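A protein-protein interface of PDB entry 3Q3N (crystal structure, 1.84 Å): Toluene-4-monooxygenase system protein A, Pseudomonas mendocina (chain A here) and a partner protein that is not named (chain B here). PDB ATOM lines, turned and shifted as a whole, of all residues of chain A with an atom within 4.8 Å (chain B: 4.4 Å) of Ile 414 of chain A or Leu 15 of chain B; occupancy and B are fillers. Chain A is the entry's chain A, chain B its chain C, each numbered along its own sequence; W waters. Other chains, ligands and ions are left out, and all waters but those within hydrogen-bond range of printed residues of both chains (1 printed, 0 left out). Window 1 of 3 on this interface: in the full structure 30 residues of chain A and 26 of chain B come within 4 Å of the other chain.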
ATOM      1  N   TRP A 338       4.216   3.107  19.331  1.00  0.00           N
ATOM      2  CA  TRP A 338       4.890   2.748  18.084  1.00  0.00           C
ATOM      3  C   TRP A 338       4.408   3.623  16.926  1.00  0.00           C
ATOM      4  O   TRP A 338       4.371   3.180  15.777  1.00  0.00           O
ATOM      5  CB  TRP A 338       4.676   1.259  17.757  1.00  0.00           C
ATOM      6  CG  TRP A 338       5.625   0.338  18.497  1.00  0.00           C
ATOM      7  CD1 TRP A 338       6.775  -0.221  18.014  1.00  0.00           C
ATOM      8  CD2 TRP A 338       5.489  -0.130  19.845  1.00  0.00           C
ATOM      9  NE1 TRP A 338       7.371  -0.994  18.982  1.00  0.00           N
ATOM     10  CE2 TRP A 338       6.600  -0.959  20.114  1.00  0.00           C
ATOM     11  CE3 TRP A 338       4.535   0.073  20.851  1.00  0.00           C
ATOM     12  CZ2 TRP A 338       6.789  -1.578  21.348  1.00  0.00           C
ATOM     13  CZ3 TRP A 338       4.724  -0.545  22.078  1.00  0.00           C
ATOM     14  CH2 TRP A 338       5.843  -1.364  22.313  1.00  0.00           C
ATOM     15  N   PRO A 394       6.632  -5.081  19.033  1.00  0.00           N
ATOM     16  CA  PRO A 394       5.610  -5.729  19.851  1.00  0.00           C
ATOM     17  C   PRO A 394       5.388  -7.134  19.331  1.00  0.00           C
ATOM     18  O   PRO A 394       5.638  -7.379  18.147  1.00  0.00           O
ATOM     19  CB  PRO A 394       4.367  -4.870  19.596  1.00  0.00           C
ATOM     20  CG  PRO A 394       4.591  -4.262  18.265  1.00  0.00           C
ATOM     21  CD  PRO A 394       6.066  -4.082  18.105  1.00  0.00           C
ATOM     22  N   LEU A 404      -0.176  -7.932  20.706  1.00  0.00           N
ATOM     23  CA  LEU A 404      -0.814  -8.732  21.751  1.00  0.00           C
ATOM     24  C   LEU A 404      -0.873  -7.923  23.045  1.00  0.00           C
ATOM     25  O   LEU A 404       0.162  -7.588  23.615  1.00  0.00           O
ATOM     26  CB  LEU A 404      -0.026 -10.029  21.977  1.00  0.00           C
ATOM     27  CG  LEU A 404       0.138 -11.043  20.836  1.00  0.00           C
ATOM     28  CD1 LEU A 404       1.080 -12.180  21.248  1.00  0.00           C
ATOM     29  CD2 LEU A 404      -1.221 -11.621  20.406  1.00  0.00           C
ATOM     30  N   VAL A 405      -2.079  -7.623  23.522  1.00  0.00           N
ATOM     31  CA  VAL A 405      -2.236  -6.701  24.650  1.00  0.00           C
ATOM     32  C   VAL A 405      -3.084  -7.249  25.798  1.00  0.00           C
ATOM     33  O   VAL A 405      -3.726  -8.291  25.671  1.00  0.00           O
ATOM     34  CB  VAL A 405      -2.854  -5.357  24.191  1.00  0.00           C
ATOM     35  CG1 VAL A 405      -1.951  -4.671  23.185  1.00  0.00           C
ATOM     36  CG2 VAL A 405      -4.254  -5.568  23.614  1.00  0.00           C
ATOM     37  N   GLY A 406      -3.085  -6.530  26.918  1.00  0.00           N
ATOM     38  CA  GLY A 406      -3.931  -6.869  28.050  1.00  0.00           C
ATOM     39  C   GLY A 406      -4.296  -5.621  28.839  1.00  0.00           C
ATOM     40  O   GLY A 406      -4.219  -4.520  28.318  1.00  0.00           O
ATOM     41  N   TRP A 412      -3.267  -5.675  36.711  1.00  0.00           N
ATOM     42  CA  TRP A 412      -2.625  -6.243  35.533  1.00  0.00           C
ATOM     43  C   TRP A 412      -3.163  -7.627  35.187  1.00  0.00           C
ATOM     44  O   TRP A 412      -3.221  -8.512  36.032  1.00  0.00           O
ATOM     45  CB  TRP A 412      -1.113  -6.331  35.772  1.00  0.00           C
ATOM     46  CG  TRP A 412      -0.323  -6.893  34.621  1.00  0.00           C
ATOM     47  CD1 TRP A 412      -0.242  -6.386  33.353  1.00  0.00           C
ATOM     48  CD2 TRP A 412       0.516  -8.057  34.642  1.00  0.00           C
ATOM     49  NE1 TRP A 412       0.592  -7.166  32.585  1.00  0.00           N
ATOM     50  CE2 TRP A 412       1.068  -8.197  33.350  1.00  0.00           C
ATOM     51  CE3 TRP A 412       0.853  -8.996  35.626  1.00  0.00           C
ATOM     52  CZ2 TRP A 412       1.935  -9.239  33.017  1.00  0.00           C
ATOM     53  CZ3 TRP A 412       1.721 -10.027  35.294  1.00  0.00           C
ATOM     54  CH2 TRP A 412       2.249 -10.142  34.000  1.00  0.00           C
ATOM     55  N   ASN A 413      -3.577  -7.798  33.937  1.00  0.00           N
ATOM     56  CA  ASN A 413      -3.901  -9.113  33.411  1.00  0.00           C
ATOM     57  C   ASN A 413      -3.688  -9.129  31.911  1.00  0.00           C
ATOM     58  O   ASN A 413      -4.195  -8.269  31.190  1.00  0.00           O
ATOM     59  CB  ASN A 413      -5.339  -9.523  33.740  1.00  0.00           C
ATOM     60  CG  ASN A 413      -5.659 -10.949  33.290  1.00  0.00           C
ATOM     61  OD1 ASN A 413      -5.283 -11.918  33.948  1.00  0.00           O
ATOM     62  ND2 ASN A 413      -6.357 -11.076  32.166  1.00  0.00           N
ATOM     63  N   ILE A 414      -2.921 -10.103  31.442  1.00  0.00           N
ATOM     64  CA  ILE A 414      -2.687 -10.244  30.014  1.00  0.00           C
ATOM     65  C   ILE A 414      -2.614 -11.719  29.659  1.00  0.00           C
ATOM     66  O   ILE A 414      -2.012 -12.508  30.389  1.00  0.00           O
ATOM     67  CB  ILE A 414      -1.411  -9.495  29.568  1.00  0.00           C
ATOM     68  CG1 ILE A 414      -1.264  -9.544  28.043  1.00  0.00           C
ATOM     69  CG2 ILE A 414      -0.168 -10.038  30.277  1.00  0.00           C
ATOM     70  CD1 ILE A 414      -0.411  -8.428  27.484  1.00  0.00           C
ATOM     71  N   GLU A 415      -3.254 -12.102  28.559  1.00  0.00           N
ATOM     72  CA  GLU A 415      -3.206 -13.501  28.144  1.00  0.00           C
ATOM     73  C   GLU A 415      -3.008 -13.691  26.648  1.00  0.00           C
ATOM     74  O   GLU A 415      -3.677 -13.066  25.824  1.00  0.00           O
ATOM     75  CB  GLU A 415      -4.447 -14.266  28.601  1.00  0.00           C
ATOM     76  CG  GLU A 415      -4.315 -15.768  28.349  1.00  0.00           C
ATOM     77  CD  GLU A 415      -5.345 -16.586  29.082  1.00  0.00           C
ATOM     78  OE1 GLU A 415      -6.214 -15.995  29.757  1.00  0.00           O
ATOM     79  OE2 GLU A 415      -5.277 -17.828  28.980  1.00  0.00           O
ATOM     80  N   VAL A 416      -2.073 -14.571  26.315  1.00  0.00           N
ATOM     81  CA  VAL A 416      -1.812 -14.954  24.942  1.00  0.00           C
ATOM     82  C   VAL A 416      -2.316 -16.378  24.785  1.00  0.00           C
ATOM     83  O   VAL A 416      -2.133 -17.201  25.676  1.00  0.00           O
ATOM     84  CB  VAL A 416      -0.308 -14.918  24.638  1.00  0.00           C
ATOM     85  CG1 VAL A 416      -0.042 -15.334  23.194  1.00  0.00           C
ATOM     86  CG2 VAL A 416       0.249 -13.526  24.912  1.00  0.00           C
ATOM     87  N   ALA B   8       7.750 -11.549  25.749  1.00  0.00           N
ATOM     88  CA  ALA B   8       7.711 -11.305  27.186  1.00  0.00           C
ATOM     89  C   ALA B   8       6.649 -10.292  27.599  1.00  0.00           C
ATOM     90  O   ALA B   8       6.559  -9.192  27.043  1.00  0.00           O
ATOM     91  CB  ALA B   8       9.108 -10.860  27.692  1.00  0.00           C
ATOM     92  N   ALA B   9       5.851 -10.676  28.590  1.00  0.00           N
ATOM     93  CA  ALA B   9       4.894  -9.771  29.208  1.00  0.00           C
ATOM     94  C   ALA B   9       5.405  -9.317  30.574  1.00  0.00           C
ATOM     95  O   ALA B   9       5.610 -10.139  31.470  1.00  0.00           O
ATOM     96  CB  ALA B   9       3.536 -10.449  29.342  1.00  0.00           C
ATOM     97  N   ASP B  13       2.559  -3.835  32.646  1.00  0.00           N
ATOM     98  CA  ASP B  13       2.605  -3.286  31.291  1.00  0.00           C
ATOM     99  C   ASP B  13       1.300  -3.621  30.571  1.00  0.00           C
ATOM    100  O   ASP B  13       0.452  -4.342  31.112  1.00  0.00           O
ATOM    101  CB  ASP B  13       3.781  -3.865  30.508  1.00  0.00           C
ATOM    102  CG  ASP B  13       4.287  -2.920  29.432  1.00  0.00           C
ATOM    103  OD1 ASP B  13       3.618  -1.894  29.154  1.00  0.00           O
ATOM    104  OD2 ASP B  13       5.359  -3.209  28.858  1.00  0.00           O
ATOM    105  N   PHE B  14       1.147  -3.115  29.349  1.00  0.00           N
ATOM    106  CA  PHE B  14      -0.084  -3.318  28.586  1.00  0.00           C
ATOM    107  C   PHE B  14       0.046  -4.328  27.451  1.00  0.00           C
ATOM    108  O   PHE B  14      -0.957  -4.699  26.847  1.00  0.00           O
ATOM    109  CB  PHE B  14      -0.592  -1.987  28.016  1.00  0.00           C
ATOM    110  CG  PHE B  14       0.050  -1.599  26.706  1.00  0.00           C
ATOM    111  CD1 PHE B  14      -0.628  -1.770  25.507  1.00  0.00           C
ATOM    112  CD2 PHE B  14       1.328  -1.065  26.673  1.00  0.00           C
ATOM    113  CE1 PHE B  14      -0.042  -1.415  24.304  1.00  0.00           C
ATOM    114  CE2 PHE B  14       1.918  -0.707  25.472  1.00  0.00           C
ATOM    115  CZ  PHE B  14       1.232  -0.881  24.289  1.00  0.00           C
ATOM    116  N   LEU B  15       1.264  -4.775  27.149  1.00  0.00           N
ATOM    117  CA  LEU B  15       1.440  -5.680  26.012  1.00  0.00           C
ATOM    118  C   LEU B  15       2.508  -6.760  26.190  1.00  0.00           C
ATOM    119  O   LEU B  15       3.232  -6.794  27.190  1.00  0.00           O
ATOM    120  CB  LEU B  15       1.746  -4.873  24.749  1.00  0.00           C
ATOM    121  CG  LEU B  15       3.225  -4.545  24.534  1.00  0.00           C
ATOM    122  CD1 LEU B  15       3.443  -3.898  23.173  1.00  0.00           C
ATOM    123  CD2 LEU B  15       3.774  -3.665  25.648  1.00  0.00           C
ATOM    124  N   VAL B  16       2.589  -7.641  25.196  1.00  0.00           N
ATOM    125  CA  VAL B  16       3.670  -8.610  25.083  1.00  0.00           C
ATOM    126  C   VAL B  16       4.644  -8.095  24.029  1.00  0.00           C
ATOM    127  O   VAL B  16       4.223  -7.635  22.972  1.00  0.00           O
ATOM    128  CB  VAL B  16       3.145 -10.012  24.643  1.00  0.00           C
ATOM    129  CG1 VAL B  16       4.255 -11.046  24.717  1.00  0.00           C
ATOM    130  CG2 VAL B  16       1.941 -10.441  25.494  1.00  0.00           C
ATOM    131  N   GLN B  17       5.944  -8.161  24.305  1.00  0.00           N
ATOM    132  CA  GLN B  17       6.935  -7.664  23.344  1.00  0.00           C
ATOM    133  C   GLN B  17       7.937  -8.734  22.938  1.00  0.00           C
ATOM    134  O   GLN B  17       8.185  -9.681  23.692  1.00  0.00           O
ATOM    135  CB  GLN B  17       7.713  -6.480  23.920  1.00  0.00           C
ATOM    136  CG  GLN B  17       6.952  -5.186  24.013  1.00  0.00           C
ATOM    137  CD  GLN B  17       7.725  -4.166  24.818  1.00  0.00           C
ATOM    138  OE1 GLN B  17       8.138  -4.438  25.950  1.00  0.00           O
ATOM    139  NE2 GLN B  17       7.965  -3.005  24.231  1.00  0.00           N
ATOM    140  N   ARG B  42       6.543   2.480  30.474  1.00  0.00           N
ATOM    141  CA  ARG B  42       5.110   2.361  30.695  1.00  0.00           C
ATOM    142  C   ARG B  42       4.808   1.779  32.067  1.00  0.00           C
ATOM    143  O   ARG B  42       3.651   1.709  32.474  1.00  0.00           O
ATOM    144  CB  ARG B  42       4.472   1.514  29.594  1.00  0.00           C
ATOM    145  CG  ARG B  42       4.576   2.143  28.219  1.00  0.00           C
ATOM    146  CD  ARG B  42       4.083   1.206  27.135  1.00  0.00           C
ATOM    147  NE  ARG B  42       4.767  -0.072  27.219  1.00  0.00           N
ATOM    148  CZ  ARG B  42       5.932  -0.347  26.642  1.00  0.00           C
ATOM    149  NH1 ARG B  42       6.472  -1.545  26.802  1.00  0.00           N
ATOM    150  NH2 ARG B  42       6.556   0.564  25.913  1.00  0.00           N
ATOM    151  N   HIS B  55       4.537 -18.255  30.475  1.00  0.00           N
ATOM    152  CA  HIS B  55       3.304 -17.463  30.477  1.00  0.00           C
ATOM    153  C   HIS B  55       2.153 -18.125  31.237  1.00  0.00           C
ATOM    154  O   HIS B  55       1.796 -19.268  30.966  1.00  0.00           O
ATOM    155  CB  HIS B  55       2.870 -17.141  29.041  1.00  0.00           C
ATOM    156  CG  HIS B  55       1.756 -16.140  28.947  1.00  0.00           C
ATOM    157  ND1 HIS B  55       0.573 -16.404  28.293  1.00  0.00           N
ATOM    158  CD2 HIS B  55       1.653 -14.875  29.418  1.00  0.00           C
ATOM    159  CE1 HIS B  55      -0.213 -15.342  28.361  1.00  0.00           C
ATOM    160  NE2 HIS B  55       0.417 -14.404  29.044  1.00  0.00           N
ATOM    161  N   ARG B  56       1.577 -17.383  32.181  1.00  0.00           N
ATOM    162  CA  ARG B  56       0.404 -17.819  32.941  1.00  0.00           C
ATOM    163  C   ARG B  56       0.727 -18.995  33.855  1.00  0.00           C
ATOM    164  O   ARG B  56      -0.171 -19.568  34.475  1.00  0.00           O
ATOM    165  CB  ARG B  56      -0.767 -18.188  32.015  1.00  0.00           C
ATOM    166  CG  ARG B  56      -1.085 -17.180  30.916  1.00  0.00           C
ATOM    167  CD  ARG B  56      -1.823 -15.942  31.426  1.00  0.00           C
ATOM    168  NE  ARG B  56      -3.065 -16.262  32.126  1.00  0.00           N
ATOM    169  CZ  ARG B  56      -3.907 -15.351  32.605  1.00  0.00           C
ATOM    170  NH1 ARG B  56      -3.651 -14.056  32.448  1.00  0.00           N
ATOM    171  NH2 ARG B  56      -5.012 -15.729  33.232  1.00  0.00           N
HETATM  172  O   HOH W   1       2.236  -7.248  30.336  1.00  0.00           O
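N of Ala 8 of chain B lies within hydrogen-bond range of O of Gln 17 of chain B, at 2.8 Å. OD2 of Asp 13 of chain B is in salt-bridge range of NH1 of Arg 42 of chain B. NH1 of Arg 42 of chain B sits close to NE2 of Gln 17 of chain B (3.3 Å).
Ile 414 of chain A touches just these residues of chain B: Ala 9, Phe 14, Leu 15, Val 16, His 55 and Arg 56. Of the printed residues of chain A, Leu 15 of chain B touches Trp 338, Pro 394, Leu 404 and Ile 414. Printed residues of chain A within 4 Å of Asp 13 of chain B: Trp 412. Printed residues of chain B within 4 Å of Val 405 of chain A: Phe 14 (3.2 Å). Printed residues of chain A within 4 Å of Ala 9 of chain B: Ile 414. Printed residues of chain A within 4 Å of His 55 of chain B: Ile 414 (3.4 Å), Glu 415 (3.5 Å) and Val 416 (2.9 Å). Printed residues of chain A within 4 Å of Phe 14 of chain B: Val 405, Gly 406 and Ile 414. Ala 8 of chain B touches none of the printed residues of chain A. Arg 42 of chain B touches none of the printed residues of chain A. The nearest printed residue of chain A that does not touch Leu 15 of chain B is Val 405 of chain A (4.02 Å). The nearest printed residue of chain B that does not touch Val 416 of chain A is Arg 56 of chain B (5.3 Å).
N of Val 16 of chain B lies within hydrogen-bond range of O of Leu 404 of chain A. The backbone NH (N) of Gly 406 of chain A lies within hydrogen-bond range of the backbone carbonyl oxygen (O) of Phe 14 of chain B, at 2.8 Å. The backbone carbonyl oxygen (O) of Asp 13 of chain B lies close to the indole nitrogen (NE1) of Trp 412 of chain A (3.2 Å). The side-chain amide oxygen of Asn 413 of chain A sits at hydrogen-bond distance from the guanidinium group of Arg 56 of chain B, 3.1 Å away. The backbone carbonyl oxygen (O) of Ile 414 of chain A sits at hydrogen-bond distance from a ring nitrogen (NE2) of His 55 of chain B (3.4 Å). The guanidinium group (NH1) of Arg 56 of chain B is in hydrogen-bond range of the backbone carbonyl oxygen (O) of Ile 414 of chain A, at 3.1 Å. The side-chain carboxylate of Glu 415 of chain A is in salt-bridge range of the guanidinium group of Arg 56 of chain B (3.7 Å).
Of the 10 printed residues of chain B, 8 touch a printed residue of chain A. Along chain B the printed residues that touch a printed residue of chain A span positions 9 to 56. Printed residues of chain A that touch a printed residue of chain B: Trp 338, Pro 394, Leu 404, Val 405, Gly 406, Trp 412, Asn 413, Ile 414, Glu 415 and Val 416. Along chain A the printed residues that touch a printed residue of chain B span positions 338 to 416. Among the printed residues, 20 pairs touch across the chains.
Water W1 lies within hydrogen-bond range of the indole nitrogen (NE1) of Trp 412 of chain A (2.8 Å), the backbone carbonyl oxygen (O) of Leu 15 of chain B (3.3 Å) and the backbone carbonyl oxygen (O) of Asp 13 of chain B (3.5 Å).
Among the printed residues, merely in contact across the chains: Trp 338 of chain A with Leu 15 of chain B (3.6 Å), Trp 338 of chain A with Gln 17 of chain B (3.3 Å), Pro 394 of chain A with Leu 15 of chain B (3.8 Å), Pro 394 of chain A with Val 16 of chain B (3.9 Å), Leu 404 of chain A with Leu 15 of chain B (3.3 Å), Val 405 of chain A with Phe 14 of chain B (3.2 Å), Ile 414 of chain A with Ala 9 of chain B (3.8 Å), Ile 414 of chain A with Phe 14 of chain B (3.8 Å), Ile 414 of chain A with Leu 15 of chain B (3.6 Å), Ile 414 of chain A with Val 16 of chain B (3.7 Å), Glu 415 of chain A with His 55 of chain B (3.5 Å), Val 416 of chain A with Val 16 of chain B (3.6 Å) and Val 416 of chain A with His 55 of chain B (2.9 Å).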
